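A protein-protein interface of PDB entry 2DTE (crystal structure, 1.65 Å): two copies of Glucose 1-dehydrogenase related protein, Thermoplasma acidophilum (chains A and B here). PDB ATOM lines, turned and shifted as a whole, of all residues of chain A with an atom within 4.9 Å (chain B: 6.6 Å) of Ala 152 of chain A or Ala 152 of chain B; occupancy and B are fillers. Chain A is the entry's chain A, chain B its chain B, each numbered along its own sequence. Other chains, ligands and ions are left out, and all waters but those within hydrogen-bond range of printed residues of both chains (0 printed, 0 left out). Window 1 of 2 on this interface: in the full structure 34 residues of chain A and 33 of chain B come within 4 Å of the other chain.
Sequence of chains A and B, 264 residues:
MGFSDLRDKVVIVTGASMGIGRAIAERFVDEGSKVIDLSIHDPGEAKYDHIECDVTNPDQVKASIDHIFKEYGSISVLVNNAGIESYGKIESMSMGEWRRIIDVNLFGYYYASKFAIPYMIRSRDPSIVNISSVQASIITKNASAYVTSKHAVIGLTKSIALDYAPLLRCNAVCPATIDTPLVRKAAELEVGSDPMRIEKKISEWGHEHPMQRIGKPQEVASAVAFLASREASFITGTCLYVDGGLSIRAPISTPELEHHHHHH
The side-chain hydroxyl (OG1) of Thr 148 of chain A is in hydrogen-bond range of the backbone NH (N) of Leu 156 of chain B.
The side-chain hydroxyl of Thr 148 of chain B lies within hydrogen-bond range of the backbone NH of Leu 156 of chain A (3.4 Å).
Of the printed residues of chain B, Leu 106 of chain A touches Thr 148.
Lys 150 of chain A touches none of the printed residues of chain B.
Ala 152 of chain A touches just these residues of chain B: Thr 148 and Ala 152.
Printed residues of chain A within 4 Å of Leu 106 of chain B: Thr 148 (3.7 Å).
Printed residues of chain A within 4 Å of Val 147 of chain B: Gly 155 (3.7 Å).
Of the printed residues of chain A, Thr 148 of chain B touches Leu 106 (3.7 Å), Ala 152 (3.5 Å), Gly 155 (3.8 Å) and Leu 156 (3.4 Å).
Ala 152 of chain B touches just these residues of chain A: Thr 148 (3.6 Å) and Ala 152 (3.9 Å).
Of the printed residues of chain A, Leu 156 of chain B touches Thr 148.
The nearest residue of chain B that does not touch Ala 152 of chain A is His 151 of chain B (4.4 Å).
The nearest residue of chain A that does not touch Ala 152 of chain B is His 151 of chain A (4.4 Å).
The nearest printed residue of chain B that does not touch Leu 156 of chain A is Val 147 of chain B (5.3 Å).
The backbone carbonyl oxygen (O) of Val 147 of chain B sits at hydrogen-bond distance from a ring nitrogen (ND1) of His 151 of chain B, at 2.9 Å.
Leu 106 of chain A touches Thr 148 of chain B, and with the chains exchanged Thr 148 of chain A touches Leu 106 of chain B.
His 151 of chain A touches its own counterpart, His 151 of chain B.
His 151 of chain A touches Gly 155 of chain B, and with the chains exchanged Gly 155 of chain A touches His 151 of chain B.
Ala 152 of chain A touches its own counterpart, Ala 152 of chain B.
Positions printed for both chains: 106, 148, 149, 150, 151, 152, 153, 154, 155 and 156.
Of the 15 pairs that touch across the chains among the printed residues, 14 have their exchanged pair printed and touching as well.
CD1 of Leu 106 of chain A touches CG2 of Thr 148 of chain B, 3.7 Å away.
Thr 148 of chain A touches Leu 106 of chain B.
CG2 of Thr 148 of chain A touches O of Ala 152 of chain B, 3.6 Å away.
CG of His 151 of chain A touches CA of Gly 155 of chain B, at 3.4 Å.
Ala 152 of chain A touches Thr 148 of chain B (O to CG2, 3.5 Å).
Ala 152 of chain A touches Ala 152 of chain B.
His 151 of chain B touches Ile 154 of chain A (CD2 to CG2, 3.9 Å).
Gly 155 of chain A touches Val 147 of chain B (O to CG1, 3.7 Å).
Thr 148 of chain B touches Gly 155 of chain A.
CG of His 151 of chain B touches CA of Gly 155 of chain A, at 3.4 Å.
Of the 14 printed residues of chain B, 8 touch a printed residue of chain A.
Among the printed residues, no Asp or Glu carboxylate lies within 4 Å of a Lys or Arg side-chain nitrogen of the other chain.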
ATOM      1  N   LEU A 106      10.995  11.567  13.354  1.00  0.00           N
ATOM      2  CA  LEU A 106      11.163  11.836  11.938  1.00  0.00           C
ATOM      3  C   LEU A 106      10.280  12.988  11.476  1.00  0.00           C
ATOM      4  O   LEU A 106      10.771  13.965  10.911  1.00  0.00           O
ATOM      5  CB  LEU A 106      10.846  10.598  11.093  1.00  0.00           C
ATOM      6  CG  LEU A 106      10.741  10.891   9.589  1.00  0.00           C
ATOM      7  CD1 LEU A 106      12.093  11.345   9.031  1.00  0.00           C
ATOM      8  CD2 LEU A 106      10.242   9.658   8.855  1.00  0.00           C
ATOM      9  N   THR A 148      14.500   2.680  13.367  1.00  0.00           N
ATOM     10  CA  THR A 148      13.931   3.035  12.072  1.00  0.00           C
ATOM     11  C   THR A 148      13.918   4.559  11.927  1.00  0.00           C
ATOM     12  O   THR A 148      14.303   5.109  10.889  1.00  0.00           O
ATOM     13  CB  THR A 148      12.490   2.490  11.950  1.00  0.00           C
ATOM     14  OG1 THR A 148      12.528   1.054  11.996  1.00  0.00           O
ATOM     15  CG2 THR A 148      11.861   2.907  10.638  1.00  0.00           C
ATOM     16  N   SER A 149      13.487   5.249  12.967  1.00  0.00           N
ATOM     17  CA  SER A 149      13.417   6.701  12.869  1.00  0.00           C
ATOM     18  C   SER A 149      14.771   7.359  12.682  1.00  0.00           C
ATOM     19  O   SER A 149      14.878   8.348  11.947  1.00  0.00           O
ATOM     20  CB  SER A 149      12.711   7.297  14.095  1.00  0.00           C
ATOM     21  OG  SER A 149      13.544   7.321  15.243  1.00  0.00           O
ATOM     22  N   LYS A 150      15.808   6.815  13.318  1.00  0.00           N
ATOM     23  CA  LYS A 150      17.127   7.423  13.210  1.00  0.00           C
ATOM     24  C   LYS A 150      17.770   7.197  11.843  1.00  0.00           C
ATOM     25  O   LYS A 150      18.523   8.043  11.366  1.00  0.00           O
ATOM     26  CB  LYS A 150      18.024   6.951  14.360  1.00  0.00           C
ATOM     27  CG  LYS A 150      17.545   7.477  15.733  1.00  0.00           C
ATOM     28  CD  LYS A 150      17.428   9.010  15.686  1.00  0.00           C
ATOM     29  CE  LYS A 150      17.125   9.628  17.046  1.00  0.00           C
ATOM     30  NZ  LYS A 150      17.142  11.132  16.981  1.00  0.00           N
ATOM     31  N   HIS A 151      17.464   6.062  11.217  1.00  0.00           N
ATOM     32  CA  HIS A 151      17.927   5.789   9.863  1.00  0.00           C
ATOM     33  C   HIS A 151      17.190   6.774   8.940  1.00  0.00           C
ATOM     34  O   HIS A 151      17.791   7.367   8.049  1.00  0.00           O
ATOM     35  CB  HIS A 151      17.586   4.343   9.448  1.00  0.00           C
ATOM     36  CG  HIS A 151      18.595   3.328   9.894  1.00  0.00           C
ATOM     37  ND1 HIS A 151      18.746   2.945  11.209  1.00  0.00           N
ATOM     38  CD2 HIS A 151      19.503   2.611   9.186  1.00  0.00           C
ATOM     39  CE1 HIS A 151      19.704   2.036  11.292  1.00  0.00           C
ATOM     40  NE2 HIS A 151      20.180   1.819  10.080  1.00  0.00           N
ATOM     41  N   ALA A 152      15.885   6.960   9.178  1.00  0.00           N
ATOM     42  CA  ALA A 152      15.074   7.873   8.375  1.00  0.00           C
ATOM     43  C   ALA A 152      15.645   9.281   8.416  1.00  0.00           C
ATOM     44  O   ALA A 152      15.688   9.961   7.387  1.00  0.00           O
ATOM     45  CB  ALA A 152      13.627   7.882   8.879  1.00  0.00           C
ATOM     46  N   VAL A 153      16.076   9.716   9.598  1.00  0.00           N
ATOM     47  CA  VAL A 153      16.665  11.050   9.754  1.00  0.00           C
ATOM     48  C   VAL A 153      17.880  11.243   8.836  1.00  0.00           C
ATOM     49  O   VAL A 153      18.093  12.332   8.308  1.00  0.00           O
ATOM     50  CB  VAL A 153      17.073  11.321  11.240  1.00  0.00           C
ATOM     51  CG1 VAL A 153      17.960  12.569  11.332  1.00  0.00           C
ATOM     52  CG2 VAL A 153      15.811  11.499  12.093  1.00  0.00           C
ATOM     53  N   ILE A 154      18.682  10.199   8.642  1.00  0.00           N
ATOM     54  CA  ILE A 154      19.832  10.311   7.752  1.00  0.00           C
ATOM     55  C   ILE A 154      19.359  10.555   6.309  1.00  0.00           C
ATOM     56  O   ILE A 154      19.927  11.382   5.599  1.00  0.00           O
ATOM     57  CB  ILE A 154      20.702   9.026   7.812  1.00  0.00           C
ATOM     58  CG1 ILE A 154      21.266   8.855   9.227  1.00  0.00           C
ATOM     59  CG2 ILE A 154      21.825   9.103   6.755  1.00  0.00           C
ATOM     60  CD1 ILE A 154      22.156  10.020   9.702  1.00  0.00           C
ATOM     61  N   GLY A 155      18.302   9.858   5.887  1.00  0.00           N
ATOM     62  CA  GLY A 155      17.790  10.046   4.541  1.00  0.00           C
ATOM     63  C   GLY A 155      17.268  11.460   4.343  1.00  0.00           C
ATOM     64  O   GLY A 155      17.513  12.087   3.319  1.00  0.00           O
ATOM     65  N   LEU A 156      16.547  11.961   5.336  1.00  0.00           N
ATOM     66  CA  LEU A 156      16.009  13.318   5.259  1.00  0.00           C
ATOM     67  C   LEU A 156      17.147  14.327   5.177  1.00  0.00           C
ATOM     68  O   LEU A 156      17.082  15.306   4.417  1.00  0.00           O
ATOM     69  CB  LEU A 156      15.154  13.599   6.488  1.00  0.00           C
ATOM     70  CG  LEU A 156      14.549  14.996   6.590  1.00  0.00           C
ATOM     71  CD1 LEU A 156      13.506  15.202   5.502  1.00  0.00           C
ATOM     72  CD2 LEU A 156      13.936  15.152   7.972  1.00  0.00           C
ATOM     73  N   ILE B 102       5.661   7.784   2.910  1.00  0.00           N
ATOM     74  CA  ILE B 102       6.186   7.112   4.101  1.00  0.00           C
ATOM     75  C   ILE B 102       5.238   5.975   4.496  1.00  0.00           C
ATOM     76  O   ILE B 102       5.674   4.899   4.891  1.00  0.00           O
ATOM     77  CB  ILE B 102       6.325   8.073   5.305  1.00  0.00           C
ATOM     78  CG1 ILE B 102       7.265   9.237   4.960  1.00  0.00           C
ATOM     79  CG2 ILE B 102       6.844   7.312   6.511  1.00  0.00           C
ATOM     80  CD1 ILE B 102       8.683   8.809   4.528  1.00  0.00           C
ATOM     81  N   LEU B 106       7.228   2.611   4.077  1.00  0.00           N
ATOM     82  CA  LEU B 106       7.729   2.189   5.378  1.00  0.00           C
ATOM     83  C   LEU B 106       6.665   1.479   6.192  1.00  0.00           C
ATOM     84  O   LEU B 106       6.868   0.341   6.613  1.00  0.00           O
ATOM     85  CB  LEU B 106       8.266   3.379   6.195  1.00  0.00           C
ATOM     86  CG  LEU B 106       8.585   3.063   7.664  1.00  0.00           C
ATOM     87  CD1 LEU B 106       9.721   2.023   7.746  1.00  0.00           C
ATOM     88  CD2 LEU B 106       8.956   4.354   8.411  1.00  0.00           C
ATOM     89  N   SER B 132      14.793  -2.169  -0.571  1.00  0.00           N
ATOM     90  CA  SER B 132      15.101  -0.774  -0.260  1.00  0.00           C
ATOM     91  C   SER B 132      15.464  -0.133  -1.596  1.00  0.00           C
ATOM     92  O   SER B 132      14.681  -0.200  -2.545  1.00  0.00           O
ATOM     93  CB  SER B 132      16.269  -0.687   0.736  1.00  0.00           C
ATOM     94  OG  SER B 132      16.589   0.671   1.030  1.00  0.00           O
ATOM     95  N   VAL B 147      13.461   9.052  -0.530  1.00  0.00           N
ATOM     96  CA  VAL B 147      14.782   8.763   0.026  1.00  0.00           C
ATOM     97  C   VAL B 147      14.698   8.455   1.519  1.00  0.00           C
ATOM     98  O   VAL B 147      15.319   7.506   2.012  1.00  0.00           O
ATOM     99  CB  VAL B 147      15.740   9.942  -0.238  1.00  0.00           C
ATOM    100  CG1 VAL B 147      17.047   9.748   0.504  1.00  0.00           C
ATOM    101  CG2 VAL B 147      16.019  10.029  -1.727  1.00  0.00           C
ATOM    102  N   THR B 148      13.905   9.241   2.237  1.00  0.00           N
ATOM    103  CA  THR B 148      13.744   9.036   3.663  1.00  0.00           C
ATOM    104  C   THR B 148      13.156   7.649   3.905  1.00  0.00           C
ATOM    105  O   THR B 148      13.620   6.908   4.776  1.00  0.00           O
ATOM    106  CB  THR B 148      12.822  10.116   4.255  1.00  0.00           C
ATOM    107  OG1 THR B 148      13.452  11.391   4.098  1.00  0.00           O
ATOM    108  CG2 THR B 148      12.567   9.863   5.720  1.00  0.00           C
ATOM    109  N   SER B 149      12.139   7.298   3.125  1.00  0.00           N
ATOM    110  CA  SER B 149      11.515   5.992   3.304  1.00  0.00           C
ATOM    111  C   SER B 149      12.480   4.836   3.066  1.00  0.00           C
ATOM    112  O   SER B 149      12.437   3.844   3.801  1.00  0.00           O
ATOM    113  CB  SER B 149      10.280   5.835   2.400  1.00  0.00           C
ATOM    114  OG  SER B 149      10.600   5.630   1.039  1.00  0.00           O
ATOM    115  N   LYS B 150      13.359   4.961   2.073  1.00  0.00           N
ATOM    116  CA  LYS B 150      14.288   3.866   1.785  1.00  0.00           C
ATOM    117  C   LYS B 150      15.361   3.714   2.856  1.00  0.00           C
ATOM    118  O   LYS B 150      15.805   2.603   3.128  1.00  0.00           O
ATOM    119  CB  LYS B 150      14.889   4.026   0.383  1.00  0.00           C
ATOM    120  CG  LYS B 150      13.839   3.806  -0.741  1.00  0.00           C
ATOM    121  CD  LYS B 150      13.160   2.427  -0.590  1.00  0.00           C
ATOM    122  CE  LYS B 150      12.061   2.170  -1.623  1.00  0.00           C
ATOM    123  NZ  LYS B 150      11.491   0.780  -1.465  1.00  0.00           N
ATOM    124  N   HIS B 151      15.782   4.823   3.460  1.00  0.00           N
ATOM    125  CA  HIS B 151      16.730   4.761   4.567  1.00  0.00           C
ATOM    126  C   HIS B 151      15.995   4.123   5.756  1.00  0.00           C
ATOM    127  O   HIS B 151      16.561   3.300   6.485  1.00  0.00           O
ATOM    128  CB  HIS B 151      17.199   6.163   4.972  1.00  0.00           C
ATOM    129  CG  HIS B 151      18.307   6.706   4.125  1.00  0.00           C
ATOM    130  ND1 HIS B 151      18.128   7.095   2.812  1.00  0.00           N
ATOM    131  CD2 HIS B 151      19.605   6.961   4.424  1.00  0.00           C
ATOM    132  CE1 HIS B 151      19.268   7.579   2.344  1.00  0.00           C
ATOM    133  NE2 HIS B 151      20.178   7.508   3.302  1.00  0.00           N
ATOM    134  N   ALA B 152      14.731   4.503   5.956  1.00  0.00           N
ATOM    135  CA  ALA B 152      13.946   3.947   7.058  1.00  0.00           C
ATOM    136  C   ALA B 152      13.849   2.420   6.936  1.00  0.00           C
ATOM    137  O   ALA B 152      13.952   1.707   7.936  1.00  0.00           O
ATOM    138  CB  ALA B 152      12.530   4.567   7.082  1.00  0.00           C
ATOM    139  N   VAL B 153      13.654   1.929   5.716  1.00  0.00           N
ATOM    140  CA  VAL B 153      13.548   0.489   5.481  1.00  0.00           C
ATOM    141  C   VAL B 153      14.793  -0.244   5.971  1.00  0.00           C
ATOM    142  O   VAL B 153      14.696  -1.351   6.492  1.00  0.00           O
ATOM    143  CB  VAL B 153      13.328   0.181   3.991  1.00  0.00           C
ATOM    144  CG1 VAL B 153      13.574  -1.315   3.719  1.00  0.00           C
ATOM    145  CG2 VAL B 153      11.888   0.547   3.600  1.00  0.00           C
ATOM    146  N   ILE B 154      15.959   0.365   5.797  1.00  0.00           N
ATOM    147  CA  ILE B 154      17.202  -0.252   6.265  1.00  0.00           C
ATOM    148  C   ILE B 154      17.167  -0.387   7.790  1.00  0.00           C
ATOM    149  O   ILE B 154      17.531  -1.433   8.343  1.00  0.00           O
ATOM    150  CB  ILE B 154      18.445   0.575   5.825  1.00  0.00           C
ATOM    151  CG1 ILE B 154      18.522   0.644   4.295  1.00  0.00           C
ATOM    152  CG2 ILE B 154      19.720  -0.027   6.427  1.00  0.00           C
ATOM    153  CD1 ILE B 154      18.489  -0.693   3.593  1.00  0.00           C
ATOM    154  N   GLY B 155      16.712   0.653   8.485  1.00  0.00           N
ATOM    155  CA  GLY B 155      16.628   0.571   9.936  1.00  0.00           C
ATOM    156  C   GLY B 155      15.660  -0.520  10.371  1.00  0.00           C
ATOM    157  O   GLY B 155      15.940  -1.281  11.299  1.00  0.00           O
ATOM    158  N   LEU B 156      14.515  -0.598   9.703  1.00  0.00           N
ATOM    159  CA  LEU B 156      13.519  -1.614  10.037  1.00  0.00           C
ATOM    160  C   LEU B 156      14.125  -3.004   9.843  1.00  0.00           C
ATOM    161  O   LEU B 156      13.948  -3.907  10.671  1.00  0.00           O
ATOM    162  CB  LEU B 156      12.285  -1.459   9.151  1.00  0.00           C
ATOM    163  CG  LEU B 156      11.184  -2.496   9.401  1.00  0.00           C
ATOM    164  CD1 LEU B 156      10.592  -2.324  10.794  1.00  0.00           C
ATOM    165  CD2 LEU B 156      10.107  -2.324   8.331  1.00  0.00           C
ATOM    166  N   THR B 157      14.857  -3.156   8.747  1.00  0.00           N
ATOM    167  CA  THR B 157      15.513  -4.413   8.407  1.00  0.00           C
ATOM    168  C   THR B 157      16.497  -4.860   9.486  1.00  0.00           C
ATOM    169  O   THR B 157      16.454  -6.007   9.942  1.00  0.00           O
ATOM    170  CB  THR B 157      16.268  -4.272   7.080  1.00  0.00           C
ATOM    171  OG1 THR B 157      15.331  -4.028   6.025  1.00  0.00           O
ATOM    172  CG2 THR B 157      17.039  -5.538   6.760  1.00  0.00           C
